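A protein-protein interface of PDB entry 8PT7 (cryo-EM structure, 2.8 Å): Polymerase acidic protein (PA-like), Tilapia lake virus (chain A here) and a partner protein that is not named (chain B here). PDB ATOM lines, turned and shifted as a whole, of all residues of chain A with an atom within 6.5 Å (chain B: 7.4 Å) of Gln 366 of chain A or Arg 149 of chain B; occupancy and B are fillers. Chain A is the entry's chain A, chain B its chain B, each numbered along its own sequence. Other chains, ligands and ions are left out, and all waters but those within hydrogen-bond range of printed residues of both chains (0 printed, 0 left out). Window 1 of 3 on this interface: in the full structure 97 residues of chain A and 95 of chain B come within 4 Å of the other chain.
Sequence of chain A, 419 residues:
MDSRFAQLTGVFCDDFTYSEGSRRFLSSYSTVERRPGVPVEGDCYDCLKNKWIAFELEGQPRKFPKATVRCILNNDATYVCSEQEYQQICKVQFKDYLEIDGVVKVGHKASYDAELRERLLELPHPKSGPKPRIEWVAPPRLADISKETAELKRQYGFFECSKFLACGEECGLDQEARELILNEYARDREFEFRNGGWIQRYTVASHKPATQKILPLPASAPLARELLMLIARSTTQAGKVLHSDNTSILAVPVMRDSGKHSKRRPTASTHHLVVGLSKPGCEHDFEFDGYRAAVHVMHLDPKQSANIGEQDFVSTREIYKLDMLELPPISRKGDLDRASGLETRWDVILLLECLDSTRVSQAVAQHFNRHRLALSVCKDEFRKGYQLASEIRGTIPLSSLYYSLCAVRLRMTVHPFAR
The guanidinium group of Arg 359 of chain A lies within hydrogen-bond range of the backbone carbonyl oxygen of Ser 15 of chain B (2.8 Å).
The side-chain amide nitrogen (NE2) of Gln 362 of chain A lies within hydrogen-bond range of the backbone carbonyl oxygen (O) of Leu 14 of chain B (3.0 Å).
The side-chain amide nitrogen of Gln 362 of chain A lies within hydrogen-bond range of the backbone carbonyl oxygen of Ser 15 of chain B (2.9 Å).
The guanidinium group (NE) of Arg 370 of chain A is in hydrogen-bond range of a ring nitrogen (ND1) of His 367 of chain A.
The backbone NH (N) of Gly 11 of chain B sits close to the side-chain sulfur (SG) of Cys 9 of chain B.
NE of Arg 149 of chain B sits at hydrogen-bond distance from O of Leu 14 of chain B.
The backbone carbonyl oxygen of Gly 16 of chain B sits at hydrogen-bond distance from the side-chain amide nitrogen of Gln 147 of chain B (3.2 Å).
The backbone carbonyl oxygen (O) of Pro 17 of chain B sits at hydrogen-bond distance from the backbone NH (N) of Gln 147 of chain B (2.4 Å).
OH of Tyr 321 of chain B lies within hydrogen-bond range of OE1 of Glu 328 of chain B (3.0 Å).
Gln 366 of chain A touches just these residues of chain B: Lys 10, Arg 149 and Gly 150.
Of chain A, only Gln 362 (3.2 Å) and Gln 366 (3.6 Å) come within 4 Å of Arg 149 of chain B.
Of the printed residues of chain A, Lys 319 of chain B touches Arg 370.
Of the printed residues of chain B, Gln 362 of chain A touches Gly 11 (3.4 Å), Leu 14 (3.0 Å), Ser 15 (2.9 Å), Gly 16 (3.9 Å), Pro 17 (3.98 Å), Arg 149 (3.2 Å) and Gly 150 (3.9 Å).
The nearest residue of chain B that does not touch Gln 366 of chain A is Asn 12 of chain B (4.3 Å).
The nearest printed residue of chain A that does not touch Lys 10 of chain B is Gln 362 of chain A (4.1 Å).
Printed residues of chain A that touch a printed residue of chain B: Arg 359, Ser 361, Gln 362, Ala 363, Val 364, Ala 365, Gln 366, Phe 368, Asn 369 and Arg 370.
Printed residues of chain B that touch a printed residue of chain A: Trp 2, Cys 9, Lys 10, Gly 11, Leu 14, Ser 15, Gly 16, Pro 17, Arg 149, Gly 150, Lys 319, Tyr 321 and Glu 328.
Among the printed residues, no Asp or Glu carboxylate lies within 4 Å of a Lys or Arg side-chain nitrogen of the other chain.
Arg 359 of chain A touches Gly 16 of chain B.
O of Ser 361 of chain A touches CZ2 of Trp 2 of chain B, 3.9 Å away.
Gln 362 of chain A touches Pro 17 of chain B (OE1 to CD, 3.98 Å).
Val 364 of chain A touches Trp 2 of chain B (CG1 to CH2, 3.6 Å).
O of Lys 10 of chain B touches CB of Ala 365 of chain A, at 3.8 Å.
CG of Gln 366 of chain A touches O of Lys 10 of chain B, 3.9 Å away.
Gly 150 of chain B touches Gln 366 of chain A.
Glu 328 of chain B touches Asn 369 of chain A (OE1 to ND2, 3.9 Å).
O of Lys 319 of chain B touches CD of Arg 370 of chain A, at 3.2 Å.
CE1 of Tyr 321 of chain B touches CG of Arg 370 of chain A (3.8 Å).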
ATOM      1  N   ARG A 359      11.733 -18.329 -19.838  1.00  0.00           N
ATOM      2  CA  ARG A 359      10.604 -19.108 -19.336  1.00  0.00           C
ATOM      3  C   ARG A 359      10.316 -20.316 -20.226  1.00  0.00           C
ATOM      4  O   ARG A 359       9.169 -20.618 -20.560  1.00  0.00           O
ATOM      5  CB  ARG A 359       9.362 -18.228 -19.196  1.00  0.00           C
ATOM      6  CG  ARG A 359       9.539 -17.051 -18.251  1.00  0.00           C
ATOM      7  CD  ARG A 359       9.387 -17.474 -16.802  1.00  0.00           C
ATOM      8  NE  ARG A 359      10.179 -16.642 -15.904  1.00  0.00           N
ATOM      9  CZ  ARG A 359       9.843 -15.417 -15.524  1.00  0.00           C
ATOM     10  NH1 ARG A 359       8.727 -14.844 -15.942  1.00  0.00           N
ATOM     11  NH2 ARG A 359      10.648 -14.750 -14.704  1.00  0.00           N
ATOM     12  N   SER A 361      10.589 -23.246 -19.252  1.00  0.00           N
ATOM     13  CA  SER A 361       9.853 -24.184 -18.416  1.00  0.00           C
ATOM     14  C   SER A 361       8.362 -24.134 -18.712  1.00  0.00           C
ATOM     15  O   SER A 361       7.677 -25.152 -18.596  1.00  0.00           O
ATOM     16  CB  SER A 361      10.114 -23.887 -16.941  1.00  0.00           C
ATOM     17  OG  SER A 361       9.268 -22.852 -16.474  1.00  0.00           O
ATOM     18  N   GLN A 362       7.843 -22.970 -19.105  1.00  0.00           N
ATOM     19  CA  GLN A 362       6.427 -22.878 -19.449  1.00  0.00           C
ATOM     20  C   GLN A 362       6.114 -23.660 -20.720  1.00  0.00           C
ATOM     21  O   GLN A 362       5.080 -24.335 -20.800  1.00  0.00           O
ATOM     22  CB  GLN A 362       6.023 -21.413 -19.605  1.00  0.00           C
ATOM     23  CG  GLN A 362       6.031 -20.646 -18.297  1.00  0.00           C
ATOM     24  CD  GLN A 362       5.826 -19.161 -18.490  1.00  0.00           C
ATOM     25  OE1 GLN A 362       5.999 -18.636 -19.588  1.00  0.00           O
ATOM     26  NE2 GLN A 362       5.454 -18.473 -17.419  1.00  0.00           N
ATOM     27  N   ALA A 363       6.988 -23.580 -21.725  1.00  0.00           N
ATOM     28  CA  ALA A 363       6.798 -24.386 -22.925  1.00  0.00           C
ATOM     29  C   ALA A 363       6.842 -25.871 -22.595  1.00  0.00           C
ATOM     30  O   ALA A 363       6.013 -26.654 -23.080  1.00  0.00           O
ATOM     31  CB  ALA A 363       7.865 -24.038 -23.963  1.00  0.00           C
ATOM     32  N   VAL A 364       7.802 -26.277 -21.760  1.00  0.00           N
ATOM     33  CA  VAL A 364       7.886 -27.681 -21.371  1.00  0.00           C
ATOM     34  C   VAL A 364       6.625 -28.098 -20.624  1.00  0.00           C
ATOM     35  O   VAL A 364       6.113 -29.204 -20.816  1.00  0.00           O
ATOM     36  CB  VAL A 364       9.151 -27.933 -20.531  1.00  0.00           C
ATOM     37  CG1 VAL A 364       9.227 -29.391 -20.111  1.00  0.00           C
ATOM     38  CG2 VAL A 364      10.392 -27.542 -21.313  1.00  0.00           C
ATOM     39  N   ALA A 365       6.108 -27.222 -19.759  1.00  0.00           N
ATOM     40  CA  ALA A 365       4.906 -27.545 -18.998  1.00  0.00           C
ATOM     41  C   ALA A 365       3.695 -27.696 -19.908  1.00  0.00           C
ATOM     42  O   ALA A 365       2.868 -28.591 -19.709  1.00  0.00           O
ATOM     43  CB  ALA A 365       4.650 -26.466 -17.948  1.00  0.00           C
ATOM     44  N   GLN A 366       3.561 -26.818 -20.904  1.00  0.00           N
ATOM     45  CA  GLN A 366       2.451 -26.942 -21.842  1.00  0.00           C
ATOM     46  C   GLN A 366       2.542 -28.243 -22.628  1.00  0.00           C
ATOM     47  O   GLN A 366       1.540 -28.956 -22.797  1.00  0.00           O
ATOM     48  CB  GLN A 366       2.430 -25.742 -22.787  1.00  0.00           C
ATOM     49  CG  GLN A 366       1.932 -24.465 -22.140  1.00  0.00           C
ATOM     50  CD  GLN A 366       2.113 -23.252 -23.027  1.00  0.00           C
ATOM     51  OE1 GLN A 366       2.358 -23.377 -24.225  1.00  0.00           O
ATOM     52  NE2 GLN A 366       1.997 -22.069 -22.439  1.00  0.00           N
ATOM     53  N   HIS A 367       3.740 -28.580 -23.110  1.00  0.00           N
ATOM     54  CA  HIS A 367       3.889 -29.829 -23.849  1.00  0.00           C
ATOM     55  C   HIS A 367       3.625 -31.031 -22.952  1.00  0.00           C
ATOM     56  O   HIS A 367       3.072 -32.038 -23.400  1.00  0.00           O
ATOM     57  CB  HIS A 367       5.277 -29.919 -24.475  1.00  0.00           C
ATOM     58  CG  HIS A 367       5.325 -30.781 -25.697  1.00  0.00           C
ATOM     59  ND1 HIS A 367       4.492 -30.584 -26.777  1.00  0.00           N
ATOM     60  CD2 HIS A 367       6.094 -31.850 -26.006  1.00  0.00           C
ATOM     61  CE1 HIS A 367       4.751 -31.490 -27.701  1.00  0.00           C
ATOM     62  NE2 HIS A 367       5.720 -32.271 -27.259  1.00  0.00           N
ATOM     63  N   PHE A 368       4.007 -30.945 -21.677  1.00  0.00           N
ATOM     64  CA  PHE A 368       3.752 -32.045 -20.755  1.00  0.00           C
ATOM     65  C   PHE A 368       2.265 -32.180 -20.453  1.00  0.00           C
ATOM     66  O   PHE A 368       1.762 -33.292 -20.269  1.00  0.00           O
ATOM     67  CB  PHE A 368       4.548 -31.841 -19.467  1.00  0.00           C
ATOM     68  CG  PHE A 368       4.493 -33.009 -18.528  1.00  0.00           C
ATOM     69  CD1 PHE A 368       4.749 -34.292 -18.979  1.00  0.00           C
ATOM     70  CD2 PHE A 368       4.189 -32.825 -17.191  1.00  0.00           C
ATOM     71  CE1 PHE A 368       4.700 -35.367 -18.118  1.00  0.00           C
ATOM     72  CE2 PHE A 368       4.140 -33.896 -16.325  1.00  0.00           C
ATOM     73  CZ  PHE A 368       4.395 -35.168 -16.789  1.00  0.00           C
ATOM     74  N   ASN A 369       1.546 -31.059 -20.388  1.00  0.00           N
ATOM     75  CA  ASN A 369       0.095 -31.127 -20.252  1.00  0.00           C
ATOM     76  C   ASN A 369      -0.526 -31.827 -21.452  1.00  0.00           C
ATOM     77  O   ASN A 369      -1.400 -32.692 -21.300  1.00  0.00           O
ATOM     78  CB  ASN A 369      -0.482 -29.720 -20.094  1.00  0.00           C
ATOM     79  CG  ASN A 369      -1.901 -29.730 -19.567  1.00  0.00           C
ATOM     80  OD1 ASN A 369      -2.187 -30.337 -18.536  1.00  0.00           O
ATOM     81  ND2 ASN A 369      -2.800 -29.057 -20.274  1.00  0.00           N
ATOM     82  N   ARG A 370      -0.073 -31.475 -22.658  1.00  0.00           N
ATOM     83  CA  ARG A 370      -0.543 -32.179 -23.847  1.00  0.00           C
ATOM     84  C   ARG A 370      -0.225 -33.667 -23.759  1.00  0.00           C
ATOM     85  O   ARG A 370      -1.062 -34.514 -24.090  1.00  0.00           O
ATOM     86  CB  ARG A 370       0.090 -31.575 -25.101  1.00  0.00           C
ATOM     87  CG  ARG A 370      -0.561 -30.290 -25.575  1.00  0.00           C
ATOM     88  CD  ARG A 370      -0.031 -29.878 -26.937  1.00  0.00           C
ATOM     89  NE  ARG A 370       1.282 -29.250 -26.852  1.00  0.00           N
ATOM     90  CZ  ARG A 370       1.487 -27.952 -26.667  1.00  0.00           C
ATOM     91  NH1 ARG A 370       0.482 -27.103 -26.539  1.00  0.00           N
ATOM     92  NH2 ARG A 370       2.735 -27.496 -26.608  1.00  0.00           N
ATOM     93  N   HIS A 371       0.986 -33.999 -23.308  1.00  0.00           N
ATOM     94  CA  HIS A 371       1.389 -35.391 -23.146  1.00  0.00           C
ATOM     95  C   HIS A 371       0.441 -36.128 -22.207  1.00  0.00           C
ATOM     96  O   HIS A 371       0.002 -37.246 -22.498  1.00  0.00           O
ATOM     97  CB  HIS A 371       2.825 -35.433 -22.616  1.00  0.00           C
ATOM     98  CG  HIS A 371       3.445 -36.798 -22.591  1.00  0.00           C
ATOM     99  ND1 HIS A 371       2.718 -37.957 -22.426  1.00  0.00           N
ATOM    100  CD2 HIS A 371       4.740 -37.180 -22.691  1.00  0.00           C
ATOM    101  CE1 HIS A 371       3.537 -38.993 -22.434  1.00  0.00           C
ATOM    102  NE2 HIS A 371       4.769 -38.549 -22.596  1.00  0.00           N
ATOM    103  N   TRP B   2       5.023 -27.899 -11.500  1.00  0.00           N
ATOM    104  CA  TRP B   2       3.890 -28.108 -12.394  1.00  0.00           C
ATOM    105  C   TRP B   2       3.800 -29.552 -12.868  1.00  0.00           C
ATOM    106  O   TRP B   2       2.713 -30.000 -13.247  1.00  0.00           O
ATOM    107  CB  TRP B   2       3.986 -27.175 -13.604  1.00  0.00           C
ATOM    108  CG  TRP B   2       5.362 -27.070 -14.186  1.00  0.00           C
ATOM    109  CD1 TRP B   2       6.277 -26.089 -13.951  1.00  0.00           C
ATOM    110  CD2 TRP B   2       5.983 -27.987 -15.095  1.00  0.00           C
ATOM    111  NE1 TRP B   2       7.427 -26.334 -14.657  1.00  0.00           N
ATOM    112  CE2 TRP B   2       7.272 -27.494 -15.368  1.00  0.00           C
ATOM    113  CE3 TRP B   2       5.573 -29.175 -15.704  1.00  0.00           C
ATOM    114  CZ2 TRP B   2       8.154 -28.147 -16.223  1.00  0.00           C
ATOM    115  CZ3 TRP B   2       6.451 -29.821 -16.552  1.00  0.00           C
ATOM    116  CH2 TRP B   2       7.726 -29.307 -16.803  1.00  0.00           C
ATOM    117  N   CYS B   9      -2.411 -28.621 -15.448  1.00  0.00           N
ATOM    118  CA  CYS B   9      -1.708 -27.383 -15.134  1.00  0.00           C
ATOM    119  C   CYS B   9      -0.854 -26.989 -16.328  1.00  0.00           C
ATOM    120  O   CYS B   9      -0.084 -27.808 -16.838  1.00  0.00           O
ATOM    121  CB  CYS B   9      -0.836 -27.546 -13.886  1.00  0.00           C
ATOM    122  SG  CYS B   9      -0.129 -26.003 -13.270  1.00  0.00           S
ATOM    123  N   LYS B  10      -0.993 -25.740 -16.768  1.00  0.00           N
ATOM    124  CA  LYS B  10      -0.231 -25.215 -17.891  1.00  0.00           C
ATOM    125  C   LYS B  10       1.035 -24.486 -17.460  1.00  0.00           C
ATOM    126  O   LYS B  10       1.776 -24.003 -18.321  1.00  0.00           O
ATOM    127  CB  LYS B  10      -1.103 -24.268 -18.720  1.00  0.00           C
ATOM    128  CG  LYS B  10      -2.385 -24.896 -19.235  1.00  0.00           C
ATOM    129  CD  LYS B  10      -2.557 -24.657 -20.726  1.00  0.00           C
ATOM    130  CE  LYS B  10      -3.733 -25.438 -21.296  1.00  0.00           C
ATOM    131  NZ  LYS B  10      -4.759 -25.770 -20.269  1.00  0.00           N
ATOM    132  N   GLY B  11       1.302 -24.394 -16.160  1.00  0.00           N
ATOM    133  CA  GLY B  11       2.467 -23.677 -15.682  1.00  0.00           C
ATOM    134  C   GLY B  11       2.406 -22.195 -15.987  1.00  0.00           C
ATOM    135  O   GLY B  11       3.392 -21.605 -16.435  1.00  0.00           O
ATOM    136  N   ASN B  12       1.249 -21.583 -15.748  1.00  0.00           N
ATOM    137  CA  ASN B  12       1.027 -20.173 -16.036  1.00  0.00           C
ATOM    138  C   ASN B  12       1.272 -19.274 -14.833  1.00  0.00           C
ATOM    139  O   ASN B  12       1.002 -18.072 -14.910  1.00  0.00           O
ATOM    140  CB  ASN B  12      -0.406 -19.964 -16.539  1.00  0.00           C
ATOM    141  CG  ASN B  12      -0.567 -20.307 -18.005  1.00  0.00           C
ATOM    142  OD1 ASN B  12       0.386 -20.703 -18.672  1.00  0.00           O
ATOM    143  ND2 ASN B  12      -1.784 -20.159 -18.513  1.00  0.00           N
ATOM    144  N   LEU B  13       1.778 -19.819 -13.725  1.00  0.00           N
ATOM    145  CA  LEU B  13       1.880 -19.034 -12.500  1.00  0.00           C
ATOM    146  C   LEU B  13       2.920 -17.925 -12.613  1.00  0.00           C
ATOM    147  O   LEU B  13       2.876 -16.963 -11.839  1.00  0.00           O
ATOM    148  CB  LEU B  13       2.207 -19.949 -11.320  1.00  0.00           C
ATOM    149  CG  LEU B  13       1.109 -20.923 -10.883  1.00  0.00           C
ATOM    150  CD1 LEU B  13       1.463 -21.545  -9.546  1.00  0.00           C
ATOM    151  CD2 LEU B  13      -0.251 -20.246 -10.805  1.00  0.00           C
ATOM    152  N   LEU B  14       3.855 -18.034 -13.549  1.00  0.00           N
ATOM    153  CA  LEU B  14       4.866 -17.010 -13.761  1.00  0.00           C
ATOM    154  C   LEU B  14       4.539 -16.180 -14.996  1.00  0.00           C
ATOM    155  O   LEU B  14       3.705 -16.554 -15.825  1.00  0.00           O
ATOM    156  CB  LEU B  14       6.255 -17.638 -13.910  1.00  0.00           C
ATOM    157  CG  LEU B  14       6.778 -18.436 -12.715  1.00  0.00           C
ATOM    158  CD1 LEU B  14       8.143 -19.019 -13.031  1.00  0.00           C
ATOM    159  CD2 LEU B  14       6.838 -17.575 -11.465  1.00  0.00           C
ATOM    160  N   SER B  15       5.209 -15.039 -15.107  1.00  0.00           N
ATOM    161  CA  SER B  15       5.027 -14.172 -16.258  1.00  0.00           C
ATOM    162  C   SER B  15       5.647 -14.797 -17.503  1.00  0.00           C
ATOM    163  O   SER B  15       6.469 -15.714 -17.429  1.00  0.00           O
ATOM    164  CB  SER B  15       5.648 -12.799 -15.999  1.00  0.00           C
ATOM    165  OG  SER B  15       5.042 -12.165 -14.889  1.00  0.00           O
ATOM    166  N   GLY B  16       5.241 -14.288 -18.657  1.00  0.00           N
ATOM    167  CA  GLY B  16       5.744 -14.779 -19.918  1.00  0.00           C
ATOM    168  C   GLY B  16       7.141 -14.279 -20.203  1.00  0.00           C
ATOM    169  O   GLY B  16       7.685 -13.401 -19.519  1.00  0.00           O
ATOM    170  N   PRO B  17       7.752 -14.845 -21.240  1.00  0.00           N
ATOM    171  CA  PRO B  17       9.127 -14.463 -21.581  1.00  0.00           C
ATOM    172  C   PRO B  17       9.217 -13.029 -22.074  1.00  0.00           C
ATOM    173  O   PRO B  17       8.269 -12.476 -22.636  1.00  0.00           O
ATOM    174  CB  PRO B  17       9.507 -15.454 -22.685  1.00  0.00           C
ATOM    175  CG  PRO B  17       8.216 -15.888 -23.271  1.00  0.00           C
ATOM    176  CD  PRO B  17       7.212 -15.856 -22.161  1.00  0.00           C
ATOM    177  N   ASP B 146       6.345  -9.878 -26.855  1.00  0.00           N
ATOM    178  CA  ASP B 146       6.926 -10.530 -25.695  1.00  0.00           C
ATOM    179  C   ASP B 146       5.831 -10.931 -24.709  1.00  0.00           C
ATOM    180  O   ASP B 146       4.641 -10.687 -24.922  1.00  0.00           O
ATOM    181  CB  ASP B 146       7.958  -9.616 -25.036  1.00  0.00           C
ATOM    182  CG  ASP B 146       7.322  -8.517 -24.206  1.00  0.00           C
ATOM    183  OD1 ASP B 146       6.147  -8.177 -24.453  1.00  0.00           O
ATOM    184  OD2 ASP B 146       8.008  -7.980 -23.310  1.00  0.00           O
ATOM    185  N   GLN B 147       6.241 -11.560 -23.609  1.00  0.00           N
ATOM    186  CA  GLN B 147       5.339 -11.992 -22.546  1.00  0.00           C
ATOM    187  C   GLN B 147       4.290 -12.978 -23.044  1.00  0.00           C
ATOM    188  O   GLN B 147       3.194 -13.060 -22.481  1.00  0.00           O
ATOM    189  CB  GLN B 147       4.657 -10.793 -21.880  1.00  0.00           C
ATOM    190  CG  GLN B 147       5.623  -9.803 -21.251  1.00  0.00           C
ATOM    191  CD  GLN B 147       5.669  -9.914 -19.741  1.00  0.00           C
ATOM    192  OE1 GLN B 147       4.676  -9.667 -19.057  1.00  0.00           O
ATOM    193  NE2 GLN B 147       6.828 -10.289 -19.210  1.00  0.00           N
ATOM    194  N   GLU B 148       4.607 -13.735 -24.090  1.00  0.00           N
ATOM    195  CA  GLU B 148       3.704 -14.747 -24.627  1.00  0.00           C
ATOM    196  C   GLU B 148       4.112 -16.100 -24.056  1.00  0.00           C
ATOM    197  O   GLU B 148       5.135 -16.666 -24.454  1.00  0.00           O
ATOM    198  CB  GLU B 148       3.748 -14.750 -26.153  1.00  0.00           C
ATOM    199  CG  GLU B 148       2.383 -14.812 -26.811  1.00  0.00           C
ATOM    200  CD  GLU B 148       2.468 -14.891 -28.322  1.00  0.00           C
ATOM    201  OE1 GLU B 148       3.588 -15.070 -28.846  1.00  0.00           O
ATOM    202  OE2 GLU B 148       1.418 -14.772 -28.987  1.00  0.00           O
ATOM    203  N   ARG B 149       3.314 -16.613 -23.124  1.00  0.00           N
ATOM    204  CA  ARG B 149       3.673 -17.836 -22.420  1.00  0.00           C
ATOM    205  C   ARG B 149       3.851 -18.993 -23.395  1.00  0.00           C
ATOM    206  O   ARG B 149       3.061 -19.174 -24.326  1.00  0.00           O
ATOM    207  CB  ARG B 149       2.600 -18.183 -21.390  1.00  0.00           C
ATOM    208  CG  ARG B 149       2.931 -17.726 -19.981  1.00  0.00           C
ATOM    209  CD  ARG B 149       1.691 -17.621 -19.117  1.00  0.00           C
ATOM    210  NE  ARG B 149       1.853 -16.638 -18.052  1.00  0.00           N
ATOM    211  CZ  ARG B 149       0.907 -15.806 -17.636  1.00  0.00           C
ATOM    212  NH1 ARG B 149      -0.304 -15.807 -18.171  1.00  0.00           N
ATOM    213  NH2 ARG B 149       1.183 -14.951 -16.657  1.00  0.00           N
ATOM    214  N   GLY B 150       4.898 -19.783 -23.171  1.00  0.00           N
ATOM    215  CA  GLY B 150       5.166 -20.951 -23.982  1.00  0.00           C
ATOM    216  C   GLY B 150       5.940 -20.699 -25.254  1.00  0.00           C
ATOM    217  O   GLY B 150       6.098 -21.628 -26.054  1.00  0.00           O
ATOM    218  N   LYS B 151       6.428 -19.480 -25.471  1.00  0.00           N
ATOM    219  CA  LYS B 151       7.192 -19.125 -26.667  1.00  0.00           C
ATOM    220  C   LYS B 151       8.480 -18.442 -26.231  1.00  0.00           C
ATOM    221  O   LYS B 151       8.560 -17.206 -26.196  1.00  0.00           O
ATOM    222  CB  LYS B 151       6.376 -18.229 -27.598  1.00  0.00           C
ATOM    223  CG  LYS B 151       5.476 -18.997 -28.555  1.00  0.00           C
ATOM    224  CD  LYS B 151       4.008 -18.670 -28.335  1.00  0.00           C
ATOM    225  CE  LYS B 151       3.111 -19.742 -28.933  1.00  0.00           C
ATOM    226  NZ  LYS B 151       3.134 -20.999 -28.136  1.00  0.00           N
ATOM    227  N   PRO B 152       9.512 -19.217 -25.887  1.00  0.00           N
ATOM    228  CA  PRO B 152      10.775 -18.589 -25.461  1.00  0.00           C
ATOM    229  C   PRO B 152      11.333 -17.623 -26.488  1.00  0.00           C
ATOM    230  O   PRO B 152      11.882 -16.577 -26.118  1.00  0.00           O
ATOM    231  CB  PRO B 152      11.704 -19.790 -25.241  1.00  0.00           C
ATOM    232  CG  PRO B 152      10.795 -20.944 -25.013  1.00  0.00           C
ATOM    233  CD  PRO B 152       9.580 -20.686 -25.840  1.00  0.00           C
ATOM    234  N   LYS B 319       1.744 -30.380 -31.855  1.00  0.00           N
ATOM    235  CA  LYS B 319       0.845 -30.058 -30.754  1.00  0.00           C
ATOM    236  C   LYS B 319      -0.502 -30.759 -30.817  1.00  0.00           C
ATOM    237  O   LYS B 319      -1.064 -31.065 -29.764  1.00  0.00           O
ATOM    238  CB  LYS B 319       0.602 -28.541 -30.696  1.00  0.00           C
ATOM    239  CG  LYS B 319       1.874 -27.712 -30.642  1.00  0.00           C
ATOM    240  CD  LYS B 319       1.578 -26.231 -30.794  1.00  0.00           C
ATOM    241  CE  LYS B 319       2.646 -25.375 -30.131  1.00  0.00           C
ATOM    242  NZ  LYS B 319       4.016 -25.929 -30.317  1.00  0.00           N
ATOM    243  N   TYR B 321      -3.373 -33.477 -30.875  1.00  0.00           N
ATOM    244  CA  TYR B 321      -3.429 -34.812 -30.297  1.00  0.00           C
ATOM    245  C   TYR B 321      -4.876 -35.284 -30.244  1.00  0.00           C
ATOM    246  O   TYR B 321      -5.806 -34.559 -30.604  1.00  0.00           O
ATOM    247  CB  TYR B 321      -2.790 -34.848 -28.903  1.00  0.00           C
ATOM    248  CG  TYR B 321      -3.470 -33.978 -27.873  1.00  0.00           C
ATOM    249  CD1 TYR B 321      -3.228 -32.614 -27.819  1.00  0.00           C
ATOM    250  CD2 TYR B 321      -4.347 -34.524 -26.947  1.00  0.00           C
ATOM    251  CE1 TYR B 321      -3.843 -31.818 -26.876  1.00  0.00           C
ATOM    252  CE2 TYR B 321      -4.966 -33.737 -26.002  1.00  0.00           C
ATOM    253  CZ  TYR B 321      -4.711 -32.385 -25.970  1.00  0.00           C
ATOM    254  OH  TYR B 321      -5.328 -31.594 -25.029  1.00  0.00           O
ATOM    255  N   GLU B 328      -9.831 -29.810 -24.971  1.00  0.00           N
ATOM    256  CA  GLU B 328      -9.055 -28.583 -24.845  1.00  0.00           C
ATOM    257  C   GLU B 328      -9.432 -27.636 -25.976  1.00  0.00           C
ATOM    258  O   GLU B 328      -9.212 -27.949 -27.150  1.00  0.00           O
ATOM    259  CB  GLU B 328      -7.557 -28.881 -24.870  1.00  0.00           C
ATOM    260  CG  GLU B 328      -6.741 -28.008 -23.934  1.00  0.00           C
ATOM    261  CD  GLU B 328      -5.255 -28.069 -24.226  1.00  0.00           C
ATOM    262  OE1 GLU B 328      -4.584 -28.989 -23.713  1.00  0.00           O
ATOM    263  OE2 GLU B 328      -4.757 -27.196 -24.968  1.00  0.00           O
ATOM    264  N   CYS B 346      -5.604 -22.919 -16.177  1.00  0.00           N
ATOM    265  CA  CYS B 346      -5.012 -21.716 -16.745  1.00  0.00           C
ATOM    266  C   CYS B 346      -4.778 -20.626 -15.708  1.00  0.00           C
ATOM    267  O   CYS B 346      -4.502 -19.483 -16.083  1.00  0.00           O
ATOM    268  CB  CYS B 346      -5.898 -21.175 -17.866  1.00  0.00           C
ATOM    269  SG  CYS B 346      -6.113 -22.311 -19.238  1.00  0.00           S
ATOM    270  N   THR B 347      -4.892 -20.946 -14.421  1.00  0.00           N
ATOM    271  CA  THR B 347      -4.666 -19.948 -13.385  1.00  0.00           C
ATOM    272  C   THR B 347      -3.295 -19.314 -13.561  1.00  0.00           C
ATOM    273  O   THR B 347      -2.286 -20.011 -13.695  1.00  0.00           O
ATOM    274  CB  THR B 347      -4.782 -20.592 -12.002  1.00  0.00           C
ATOM    275  OG1 THR B 347      -6.105 -21.111 -11.822  1.00  0.00           O
ATOM    276  CG2 THR B 347      -4.491 -19.574 -10.910  1.00  0.00           C
ATOM    277  N   ALA B 348      -3.265 -17.985 -13.563  1.00  0.00           N
ATOM    278  CA  ALA B 348      -2.050 -17.222 -13.803  1.00  0.00           C
ATOM    279  C   ALA B 348      -1.715 -16.381 -12.580  1.00  0.00           C
ATOM    280  O   ALA B 348      -2.603 -15.793 -11.957  1.00  0.00           O
ATOM    281  CB  ALA B 348      -2.206 -16.319 -15.029  1.00  0.00           C
ATOM    282  N   GLY B 349      -0.430 -16.331 -12.243  1.00  0.00           N
ATOM    283  CA  GLY B 349       0.000 -15.534 -11.117  1.00  0.00           C
ATOM    284  C   GLY B 349      -0.040 -14.049 -11.419  1.00  0.00           C
ATOM    285  O   GLY B 349      -0.105 -13.615 -12.569  1.00  0.00           O
ATOM    286  N   VAL B 350      -0.003 -13.258 -10.353  1.00  0.00           N
ATOM    287  CA  VAL B 350      -0.050 -11.803 -10.438  1.00  0.00           C
ATOM    288  C   VAL B 350       1.346 -11.274 -10.110  1.00  0.00           C
ATOM    289  O   VAL B 350       1.810 -11.427  -8.971  1.00  0.00           O
ATOM    290  CB  VAL B 350      -1.103 -11.217  -9.490  1.00  0.00           C
ATOM    291  CG1 VAL B 350      -1.243  -9.721  -9.712  1.00  0.00           C
ATOM    292  CG2 VAL B 350      -2.436 -11.918  -9.687  1.00  0.00           C
ATOM    293  N   PRO B 351       2.050 -10.656 -11.055  1.00  0.00           N
ATOM    294  CA  PRO B 351       3.363 -10.084 -10.739  1.00  0.00           C
ATOM    295  C   PRO B 351       3.226  -8.821  -9.900  1.00  0.00           C
ATOM    296  O   PRO B 351       2.154  -8.231  -9.770  1.00  0.00           O
ATOM    297  CB  PRO B 351       3.964  -9.786 -12.114  1.00  0.00           C
ATOM    298  CG  PRO B 351       2.793  -9.586 -12.997  1.00  0.00           C
ATOM    299  CD  PRO B 351       1.706 -10.481 -12.478  1.00  0.00           C
